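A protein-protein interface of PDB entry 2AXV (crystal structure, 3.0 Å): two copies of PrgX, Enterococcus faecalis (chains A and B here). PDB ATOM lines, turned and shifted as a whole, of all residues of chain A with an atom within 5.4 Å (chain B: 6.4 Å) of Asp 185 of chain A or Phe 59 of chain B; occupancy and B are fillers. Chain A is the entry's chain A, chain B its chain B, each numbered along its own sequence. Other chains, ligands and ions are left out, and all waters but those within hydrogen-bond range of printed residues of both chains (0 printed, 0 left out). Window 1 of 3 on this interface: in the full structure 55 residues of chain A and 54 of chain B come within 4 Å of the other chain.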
ATOM      1  N   PHE A  59     -18.073  24.286  31.628  1.00  0.00           N
ATOM      2  CA  PHE A  59     -18.575  23.266  30.666  1.00  0.00           C
ATOM      3  C   PHE A  59     -17.907  21.931  30.849  1.00  0.00           C
ATOM      4  O   PHE A  59     -18.522  20.924  30.542  1.00  0.00           O
ATOM      5  CB  PHE A  59     -18.461  23.641  29.169  1.00  0.00           C
ATOM      6  CG  PHE A  59     -19.454  24.666  28.712  1.00  0.00           C
ATOM      7  CD1 PHE A  59     -20.808  24.361  28.639  1.00  0.00           C
ATOM      8  CD2 PHE A  59     -19.028  25.957  28.355  1.00  0.00           C
ATOM      9  CE1 PHE A  59     -21.727  25.356  28.227  1.00  0.00           C
ATOM     10  CE2 PHE A  59     -19.922  26.928  27.974  1.00  0.00           C
ATOM     11  CZ  PHE A  59     -21.264  26.647  27.911  1.00  0.00           C
ATOM     12  N   LEU A  62     -19.928  20.181  33.578  1.00  0.00           N
ATOM     13  CA  LEU A  62     -21.175  19.710  32.945  1.00  0.00           C
ATOM     14  C   LEU A  62     -20.967  18.453  32.116  1.00  0.00           C
ATOM     15  O   LEU A  62     -21.802  17.553  32.093  1.00  0.00           O
ATOM     16  CB  LEU A  62     -21.732  20.810  32.022  1.00  0.00           C
ATOM     17  CG  LEU A  62     -23.177  21.260  32.223  1.00  0.00           C
ATOM     18  CD1 LEU A  62     -23.619  21.178  33.667  1.00  0.00           C
ATOM     19  CD2 LEU A  62     -23.353  22.678  31.753  1.00  0.00           C
ATOM     20  N   ASN A  63     -19.845  18.430  31.416  1.00  0.00           N
ATOM     21  CA  ASN A  63     -19.494  17.318  30.580  1.00  0.00           C
ATOM     22  C   ASN A  63     -19.016  16.097  31.342  1.00  0.00           C
ATOM     23  O   ASN A  63     -19.272  14.974  30.925  1.00  0.00           O
ATOM     24  CB  ASN A  63     -18.428  17.736  29.562  1.00  0.00           C
ATOM     25  CG  ASN A  63     -19.020  18.096  28.209  1.00  0.00           C
ATOM     26  OD1 ASN A  63     -18.291  18.375  27.277  1.00  0.00           O
ATOM     27  ND2 ASN A  63     -20.348  18.026  28.087  1.00  0.00           N
ATOM     28  N   MET A  67     -23.039  15.139  30.386  1.00  0.00           N
ATOM     29  CA  MET A  67     -23.669  15.784  29.184  1.00  0.00           C
ATOM     30  C   MET A  67     -22.818  15.645  27.904  1.00  0.00           C
ATOM     31  O   MET A  67     -23.335  15.838  26.792  1.00  0.00           O
ATOM     32  CB  MET A  67     -24.011  17.231  29.442  1.00  0.00           C
ATOM     33  CG  MET A  67     -24.938  17.369  30.609  1.00  0.00           C
ATOM     34  SD  MET A  67     -25.652  18.997  30.576  1.00  0.00           S
ATOM     35  CE  MET A  67     -26.592  18.873  29.013  1.00  0.00           C
ATOM     36  N   PHE A 182     -21.454  31.170  19.411  1.00  0.00           N
ATOM     37  CA  PHE A 182     -22.128  30.682  20.606  1.00  0.00           C
ATOM     38  C   PHE A 182     -21.539  29.357  21.064  1.00  0.00           C
ATOM     39  O   PHE A 182     -22.262  28.421  21.358  1.00  0.00           O
ATOM     40  CB  PHE A 182     -23.601  30.540  20.296  1.00  0.00           C
ATOM     41  CG  PHE A 182     -24.299  31.866  20.135  1.00  0.00           C
ATOM     42  CD1 PHE A 182     -24.273  32.818  21.168  1.00  0.00           C
ATOM     43  CD2 PHE A 182     -24.985  32.178  18.979  1.00  0.00           C
ATOM     44  CE1 PHE A 182     -24.919  34.042  21.046  1.00  0.00           C
ATOM     45  CE2 PHE A 182     -25.653  33.422  18.885  1.00  0.00           C
ATOM     46  CZ  PHE A 182     -25.609  34.337  19.923  1.00  0.00           C
ATOM     47  N   GLY A 183     -20.206  29.301  21.096  1.00  0.00           N
ATOM     48  CA  GLY A 183     -19.466  28.136  21.534  1.00  0.00           C
ATOM     49  C   GLY A 183     -18.930  27.338  20.365  1.00  0.00           C
ATOM     50  O   GLY A 183     -19.435  27.431  19.260  1.00  0.00           O
ATOM     51  N   LYS A 184     -17.918  26.521  20.616  1.00  0.00           N
ATOM     52  CA  LYS A 184     -17.268  25.785  19.548  1.00  0.00           C
ATOM     53  C   LYS A 184     -18.247  24.849  18.868  1.00  0.00           C
ATOM     54  O   LYS A 184     -18.153  24.626  17.673  1.00  0.00           O
ATOM     55  CB  LYS A 184     -16.071  24.939  20.014  1.00  0.00           C
ATOM     56  CG  LYS A 184     -15.149  25.455  21.150  1.00  0.00           C
ATOM     57  CD  LYS A 184     -14.004  26.346  20.702  1.00  0.00           C
ATOM     58  CE  LYS A 184     -12.942  26.517  21.796  1.00  0.00           C
ATOM     59  NZ  LYS A 184     -12.410  25.164  22.069  1.00  0.00           N
ATOM     60  N   ASP A 185     -19.180  24.279  19.618  1.00  0.00           N
ATOM     61  CA  ASP A 185     -20.235  23.415  19.040  1.00  0.00           C
ATOM     62  C   ASP A 185     -21.026  24.157  17.950  1.00  0.00           C
ATOM     63  O   ASP A 185     -21.094  23.704  16.827  1.00  0.00           O
ATOM     64  CB  ASP A 185     -21.179  22.938  20.150  1.00  0.00           C
ATOM     65  CG  ASP A 185     -20.555  21.862  21.086  1.00  0.00           C
ATOM     66  OD1 ASP A 185     -21.259  21.458  22.072  1.00  0.00           O
ATOM     67  OD2 ASP A 185     -19.409  21.387  20.841  1.00  0.00           O
ATOM     68  N   TYR A 186     -21.574  25.314  18.305  1.00  0.00           N
ATOM     69  CA  TYR A 186     -22.272  26.155  17.364  1.00  0.00           C
ATOM     70  C   TYR A 186     -21.375  26.519  16.187  1.00  0.00           C
ATOM     71  O   TYR A 186     -21.806  26.411  15.031  1.00  0.00           O
ATOM     72  CB  TYR A 186     -22.717  27.416  18.063  1.00  0.00           C
ATOM     73  CG  TYR A 186     -23.352  28.425  17.161  1.00  0.00           C
ATOM     74  CD1 TYR A 186     -22.608  29.458  16.600  1.00  0.00           C
ATOM     75  CD2 TYR A 186     -24.697  28.378  16.910  1.00  0.00           C
ATOM     76  CE1 TYR A 186     -23.206  30.433  15.805  1.00  0.00           C
ATOM     77  CE2 TYR A 186     -25.320  29.333  16.112  1.00  0.00           C
ATOM     78  CZ  TYR A 186     -24.568  30.364  15.562  1.00  0.00           C
ATOM     79  OH  TYR A 186     -25.190  31.286  14.750  1.00  0.00           O
ATOM     80  N   ASP A 187     -20.143  26.951  16.495  1.00  0.00           N
ATOM     81  CA  ASP A 187     -19.186  27.421  15.511  1.00  0.00           C
ATOM     82  C   ASP A 187     -18.999  26.390  14.444  1.00  0.00           C
ATOM     83  O   ASP A 187     -18.912  26.696  13.260  1.00  0.00           O
ATOM     84  CB  ASP A 187     -17.819  27.677  16.160  1.00  0.00           C
ATOM     85  CG  ASP A 187     -17.877  28.787  17.174  1.00  0.00           C
ATOM     86  OD1 ASP A 187     -18.954  29.455  17.226  1.00  0.00           O
ATOM     87  OD2 ASP A 187     -16.880  28.973  17.931  1.00  0.00           O
ATOM     88  N   LEU A 188     -18.912  25.147  14.854  1.00  0.00           N
ATOM     89  CA  LEU A 188     -18.645  24.114  13.886  1.00  0.00           C
ATOM     90  C   LEU A 188     -19.850  23.892  12.999  1.00  0.00           C
ATOM     91  O   LEU A 188     -19.715  23.669  11.817  1.00  0.00           O
ATOM     92  CB  LEU A 188     -18.250  22.835  14.575  1.00  0.00           C
ATOM     93  CG  LEU A 188     -18.184  21.584  13.697  1.00  0.00           C
ATOM     94  CD1 LEU A 188     -17.252  21.687  12.498  1.00  0.00           C
ATOM     95  CD2 LEU A 188     -17.755  20.407  14.613  1.00  0.00           C
ATOM     96  N   THR A 189     -21.032  23.986  13.560  1.00  0.00           N
ATOM     97  CA  THR A 189     -22.218  23.725  12.780  1.00  0.00           C
ATOM     98  C   THR A 189     -22.375  24.728  11.638  1.00  0.00           C
ATOM     99  O   THR A 189     -22.475  24.318  10.452  1.00  0.00           O
ATOM    100  CB  THR A 189     -23.448  23.766  13.657  1.00  0.00           C
ATOM    101  OG1 THR A 189     -23.215  22.910  14.776  1.00  0.00           O
ATOM    102  CG2 THR A 189     -24.660  23.291  12.895  1.00  0.00           C
ATOM    103  N   SER B  51     -34.344  22.610  26.618  1.00  0.00           N
ATOM    104  CA  SER B  51     -33.528  22.541  25.429  1.00  0.00           C
ATOM    105  C   SER B  51     -34.030  21.446  24.522  1.00  0.00           C
ATOM    106  O   SER B  51     -34.238  21.709  23.341  1.00  0.00           O
ATOM    107  CB  SER B  51     -32.083  22.279  25.773  1.00  0.00           C
ATOM    108  OG  SER B  51     -31.593  23.362  26.535  1.00  0.00           O
ATOM    109  N   VAL B  56     -33.164  23.197  20.235  1.00  0.00           N
ATOM    110  CA  VAL B  56     -31.879  23.851  20.098  1.00  0.00           C
ATOM    111  C   VAL B  56     -30.998  23.450  21.251  1.00  0.00           C
ATOM    112  O   VAL B  56     -31.465  23.198  22.341  1.00  0.00           O
ATOM    113  CB  VAL B  56     -32.028  25.402  19.902  1.00  0.00           C
ATOM    114  CG1 VAL B  56     -33.473  25.794  19.623  1.00  0.00           C
ATOM    115  CG2 VAL B  56     -31.495  26.215  21.071  1.00  0.00           C
ATOM    116  N   ASN B  57     -29.706  23.426  20.991  1.00  0.00           N
ATOM    117  CA  ASN B  57     -28.752  22.658  21.815  1.00  0.00           C
ATOM    118  C   ASN B  57     -28.474  23.339  23.125  1.00  0.00           C
ATOM    119  O   ASN B  57     -28.425  24.574  23.208  1.00  0.00           O
ATOM    120  CB  ASN B  57     -27.498  22.347  21.035  1.00  0.00           C
ATOM    121  CG  ASN B  57     -27.820  21.591  19.719  1.00  0.00           C
ATOM    122  OD1 ASN B  57     -28.494  22.126  18.795  1.00  0.00           O
ATOM    123  ND2 ASN B  57     -27.356  20.346  19.637  1.00  0.00           N
ATOM    124  N   PHE B  58     -28.391  22.524  24.167  1.00  0.00           N
ATOM    125  CA  PHE B  58     -28.239  23.022  25.532  1.00  0.00           C
ATOM    126  C   PHE B  58     -27.122  24.074  25.650  1.00  0.00           C
ATOM    127  O   PHE B  58     -27.342  25.164  26.174  1.00  0.00           O
ATOM    128  CB  PHE B  58     -28.015  21.817  26.443  1.00  0.00           C
ATOM    129  CG  PHE B  58     -27.922  22.142  27.883  1.00  0.00           C
ATOM    130  CD1 PHE B  58     -26.740  22.085  28.532  1.00  0.00           C
ATOM    131  CD2 PHE B  58     -29.030  22.493  28.597  1.00  0.00           C
ATOM    132  CE1 PHE B  58     -26.680  22.375  29.870  1.00  0.00           C
ATOM    133  CE2 PHE B  58     -28.951  22.792  29.936  1.00  0.00           C
ATOM    134  CZ  PHE B  58     -27.793  22.727  30.564  1.00  0.00           C
ATOM    135  N   PHE B  59     -25.956  23.767  25.082  1.00  0.00           N
ATOM    136  CA  PHE B  59     -24.818  24.639  25.193  1.00  0.00           C
ATOM    137  C   PHE B  59     -24.996  25.921  24.432  1.00  0.00           C
ATOM    138  O   PHE B  59     -24.573  26.971  24.911  1.00  0.00           O
ATOM    139  CB  PHE B  59     -23.565  23.910  24.717  1.00  0.00           C
ATOM    140  CG  PHE B  59     -23.090  22.792  25.633  1.00  0.00           C
ATOM    141  CD1 PHE B  59     -23.594  22.613  26.911  1.00  0.00           C
ATOM    142  CD2 PHE B  59     -22.102  21.947  25.213  1.00  0.00           C
ATOM    143  CE1 PHE B  59     -23.156  21.601  27.711  1.00  0.00           C
ATOM    144  CE2 PHE B  59     -21.652  20.936  26.028  1.00  0.00           C
ATOM    145  CZ  PHE B  59     -22.179  20.772  27.279  1.00  0.00           C
ATOM    146  N   GLU B  60     -25.619  25.848  23.263  1.00  0.00           N
ATOM    147  CA  GLU B  60     -25.900  27.045  22.509  1.00  0.00           C
ATOM    148  C   GLU B  60     -26.772  27.975  23.324  1.00  0.00           C
ATOM    149  O   GLU B  60     -26.551  29.175  23.331  1.00  0.00           O
ATOM    150  CB  GLU B  60     -26.552  26.701  21.188  1.00  0.00           C
ATOM    151  CG  GLU B  60     -27.120  27.910  20.462  1.00  0.00           C
ATOM    152  CD  GLU B  60     -27.470  27.628  19.030  1.00  0.00           C
ATOM    153  OE1 GLU B  60     -28.060  28.522  18.386  1.00  0.00           O
ATOM    154  OE2 GLU B  60     -27.150  26.518  18.528  1.00  0.00           O
ATOM    155  N   ILE B  61     -27.756  27.418  24.021  1.00  0.00           N
ATOM    156  CA  ILE B  61     -28.663  28.258  24.806  1.00  0.00           C
ATOM    157  C   ILE B  61     -27.885  28.939  25.900  1.00  0.00           C
ATOM    158  O   ILE B  61     -28.022  30.138  26.067  1.00  0.00           O
ATOM    159  CB  ILE B  61     -29.865  27.500  25.415  1.00  0.00           C
ATOM    160  CG1 ILE B  61     -30.878  27.123  24.331  1.00  0.00           C
ATOM    161  CG2 ILE B  61     -30.569  28.399  26.422  1.00  0.00           C
ATOM    162  CD1 ILE B  61     -31.773  25.989  24.694  1.00  0.00           C
ATOM    163  N   LEU B  62     -27.073  28.180  26.640  1.00  0.00           N
ATOM    164  CA  LEU B  62     -26.246  28.758  27.699  1.00  0.00           C
ATOM    165  C   LEU B  62     -25.330  29.858  27.209  1.00  0.00           C
ATOM    166  O   LEU B  62     -25.107  30.831  27.920  1.00  0.00           O
ATOM    167  CB  LEU B  62     -25.431  27.679  28.385  1.00  0.00           C
ATOM    168  CG  LEU B  62     -26.246  26.782  29.331  1.00  0.00           C
ATOM    169  CD1 LEU B  62     -25.621  25.405  29.455  1.00  0.00           C
ATOM    170  CD2 LEU B  62     -26.376  27.378  30.704  1.00  0.00           C
ATOM    171  N   ASN B  63     -24.829  29.703  25.995  1.00  0.00           N
ATOM    172  CA  ASN B  63     -23.991  30.687  25.391  1.00  0.00           C
ATOM    173  C   ASN B  63     -24.750  31.903  24.873  1.00  0.00           C
ATOM    174  O   ASN B  63     -24.249  33.005  24.929  1.00  0.00           O
ATOM    175  CB  ASN B  63     -23.159  30.006  24.316  1.00  0.00           C
ATOM    176  CG  ASN B  63     -22.017  29.206  24.911  1.00  0.00           C
ATOM    177  OD1 ASN B  63     -21.483  28.281  24.285  1.00  0.00           O
ATOM    178  ND2 ASN B  63     -21.622  29.577  26.134  1.00  0.00           N
ATOM    179  N   ARG B  64     -25.965  31.729  24.402  1.00  0.00           N
ATOM    180  CA  ARG B  64     -26.812  32.868  24.083  1.00  0.00           C
ATOM    181  C   ARG B  64     -27.229  33.599  25.339  1.00  0.00           C
ATOM    182  O   ARG B  64     -27.453  34.795  25.340  1.00  0.00           O
ATOM    183  CB  ARG B  64     -28.053  32.400  23.361  1.00  0.00           C
ATOM    184  CG  ARG B  64     -27.734  31.994  21.984  1.00  0.00           C
ATOM    185  CD  ARG B  64     -28.732  31.045  21.423  1.00  0.00           C
ATOM    186  NE  ARG B  64     -28.459  30.874  20.007  1.00  0.00           N
ATOM    187  CZ  ARG B  64     -28.791  31.761  19.081  1.00  0.00           C
ATOM    188  NH1 ARG B  64     -29.405  32.895  19.403  1.00  0.00           N
ATOM    189  NH2 ARG B  64     -28.515  31.505  17.814  1.00  0.00           N
ATOM    190  N   GLY B 183     -15.444  17.826  25.889  1.00  0.00           N
ATOM    191  CA  GLY B 183     -15.898  18.951  25.060  1.00  0.00           C
ATOM    192  C   GLY B 183     -14.805  19.529  24.219  1.00  0.00           C
ATOM    193  O   GLY B 183     -13.636  19.328  24.492  1.00  0.00           O
ATOM    194  N   LYS B 184     -15.196  20.295  23.220  1.00  0.00           N
ATOM    195  CA  LYS B 184     -14.202  20.840  22.312  1.00  0.00           C
ATOM    196  C   LYS B 184     -13.287  21.842  23.090  1.00  0.00           C
ATOM    197  O   LYS B 184     -12.074  21.926  22.801  1.00  0.00           O
ATOM    198  CB  LYS B 184     -14.803  21.466  21.022  1.00  0.00           C
ATOM    199  CG  LYS B 184     -16.203  20.996  20.562  1.00  0.00           C
ATOM    200  CD  LYS B 184     -16.243  20.024  19.404  1.00  0.00           C
ATOM    201  CE  LYS B 184     -17.480  20.300  18.570  1.00  0.00           C
ATOM    202  NZ  LYS B 184     -17.535  21.796  18.332  1.00  0.00           N
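The backbone carbonyl oxygen (O) of Phe 182 of chain A lies close to the side-chain amide oxygen (OD1) of Asn 63 of chain B, 3.0 Å away.
The side-chain amino group (NZ) of Lys 184 of chain B lies within salt-bridge range of the side-chain carboxylate (OD2) of Asp 185 of chain A (3.2 Å).
NZ of Lys 184 of chain B is in hydrogen-bond range of O of Lys 184 of chain A.
OD1 of Asn 63 of chain A lies within hydrogen-bond range of N of Gly 183 of chain B (3.2 Å).
The backbone NH (N) of Met 67 of chain A sits at hydrogen-bond distance from the backbone carbonyl oxygen (O) of Leu 62 of chain A (3.2 Å).
The backbone carbonyl oxygen of Asp 185 of chain A lies within hydrogen-bond range of the side-chain hydroxyl of Thr 189 of chain A.
The side-chain amide oxygen (OD1) of Asn 63 of chain B lies close to the backbone carbonyl oxygen (O) of Phe 59 of chain B.
The guanidinium group (NE) of Arg 64 of chain B lies within salt-bridge range of the side-chain carboxylate (OE1) of Glu 60 of chain B (2.9 Å).
Phe 59 of chain A touches Phe 59 of chain B.
ND2 of Asn 63 of chain B touches CZ of Phe 59 of chain A, 3.4 Å away.
CE1 of Phe 58 of chain B touches CD2 of Leu 62 of chain A, at 3.8 Å.
ND2 of Asn 63 of chain A touches CZ of Phe 59 of chain B, at 3.4 Å.
Phe 58 of chain B touches Met 67 of chain A.
Arg 64 of chain B touches Phe 182 of chain A.
CA of Gly 183 of chain A touches OD1 of Asn 63 of chain B, at 3.4 Å.
Asp 185 of chain A touches Phe 59 of chain B (OD1 to CD2, 3.3 Å).
Tyr 186 of chain A touches Glu 60 of chain B.
Leu 188 of chain A touches Lys 184 of chain B.
Of chain A, only Phe 59, Asn 63 and Asp 185 come within 4 Å of Phe 59 of chain B.
Of the printed residues of chain B, Gly 183 of chain A touches Asn 63.
Of the printed residues of chain B, Leu 62 of chain A touches Phe 58.
Of the printed residues of chain B, Met 67 of chain A touches Phe 58.
Ser 51 of chain B touches none of the printed residues of chain A.
The nearest printed residue of chain B that does not touch Phe 182 of chain A is Glu 60 of chain B (4.1 Å).
Hydrophobic or aromatic side chains of chain A within 4 Å of the printed part of chain B: Phe 59, Leu 62, Met 67, Phe 182, Tyr 186 and Leu 188.
Along chain A the printed residues that touch a printed residue of chain B span positions 59 to 188.
Of the 12 printed residues of chain B, 7 touch a printed residue of chain A.
Printed residues of chain B that touch a printed residue of chain A: Phe 58, Phe 59, Glu 60, Asn 63, Arg 64, Gly 183 and Lys 184.
Phe 59 of chain B touches its own counterpart, Phe 59 of chain A.
Phe 59 of chain A touches Asn 63 of chain B, and with the chains exchanged Asn 63 of chain A touches Phe 59 of chain B.
Asn 63 of chain A touches Gly 183 of chain B, and with the chains exchanged Gly 183 of chain A touches Asn 63 of chain B.
Lys 184 of chain B touches its own counterpart, Lys 184 of chain A.
5 positions are printed for both chains.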
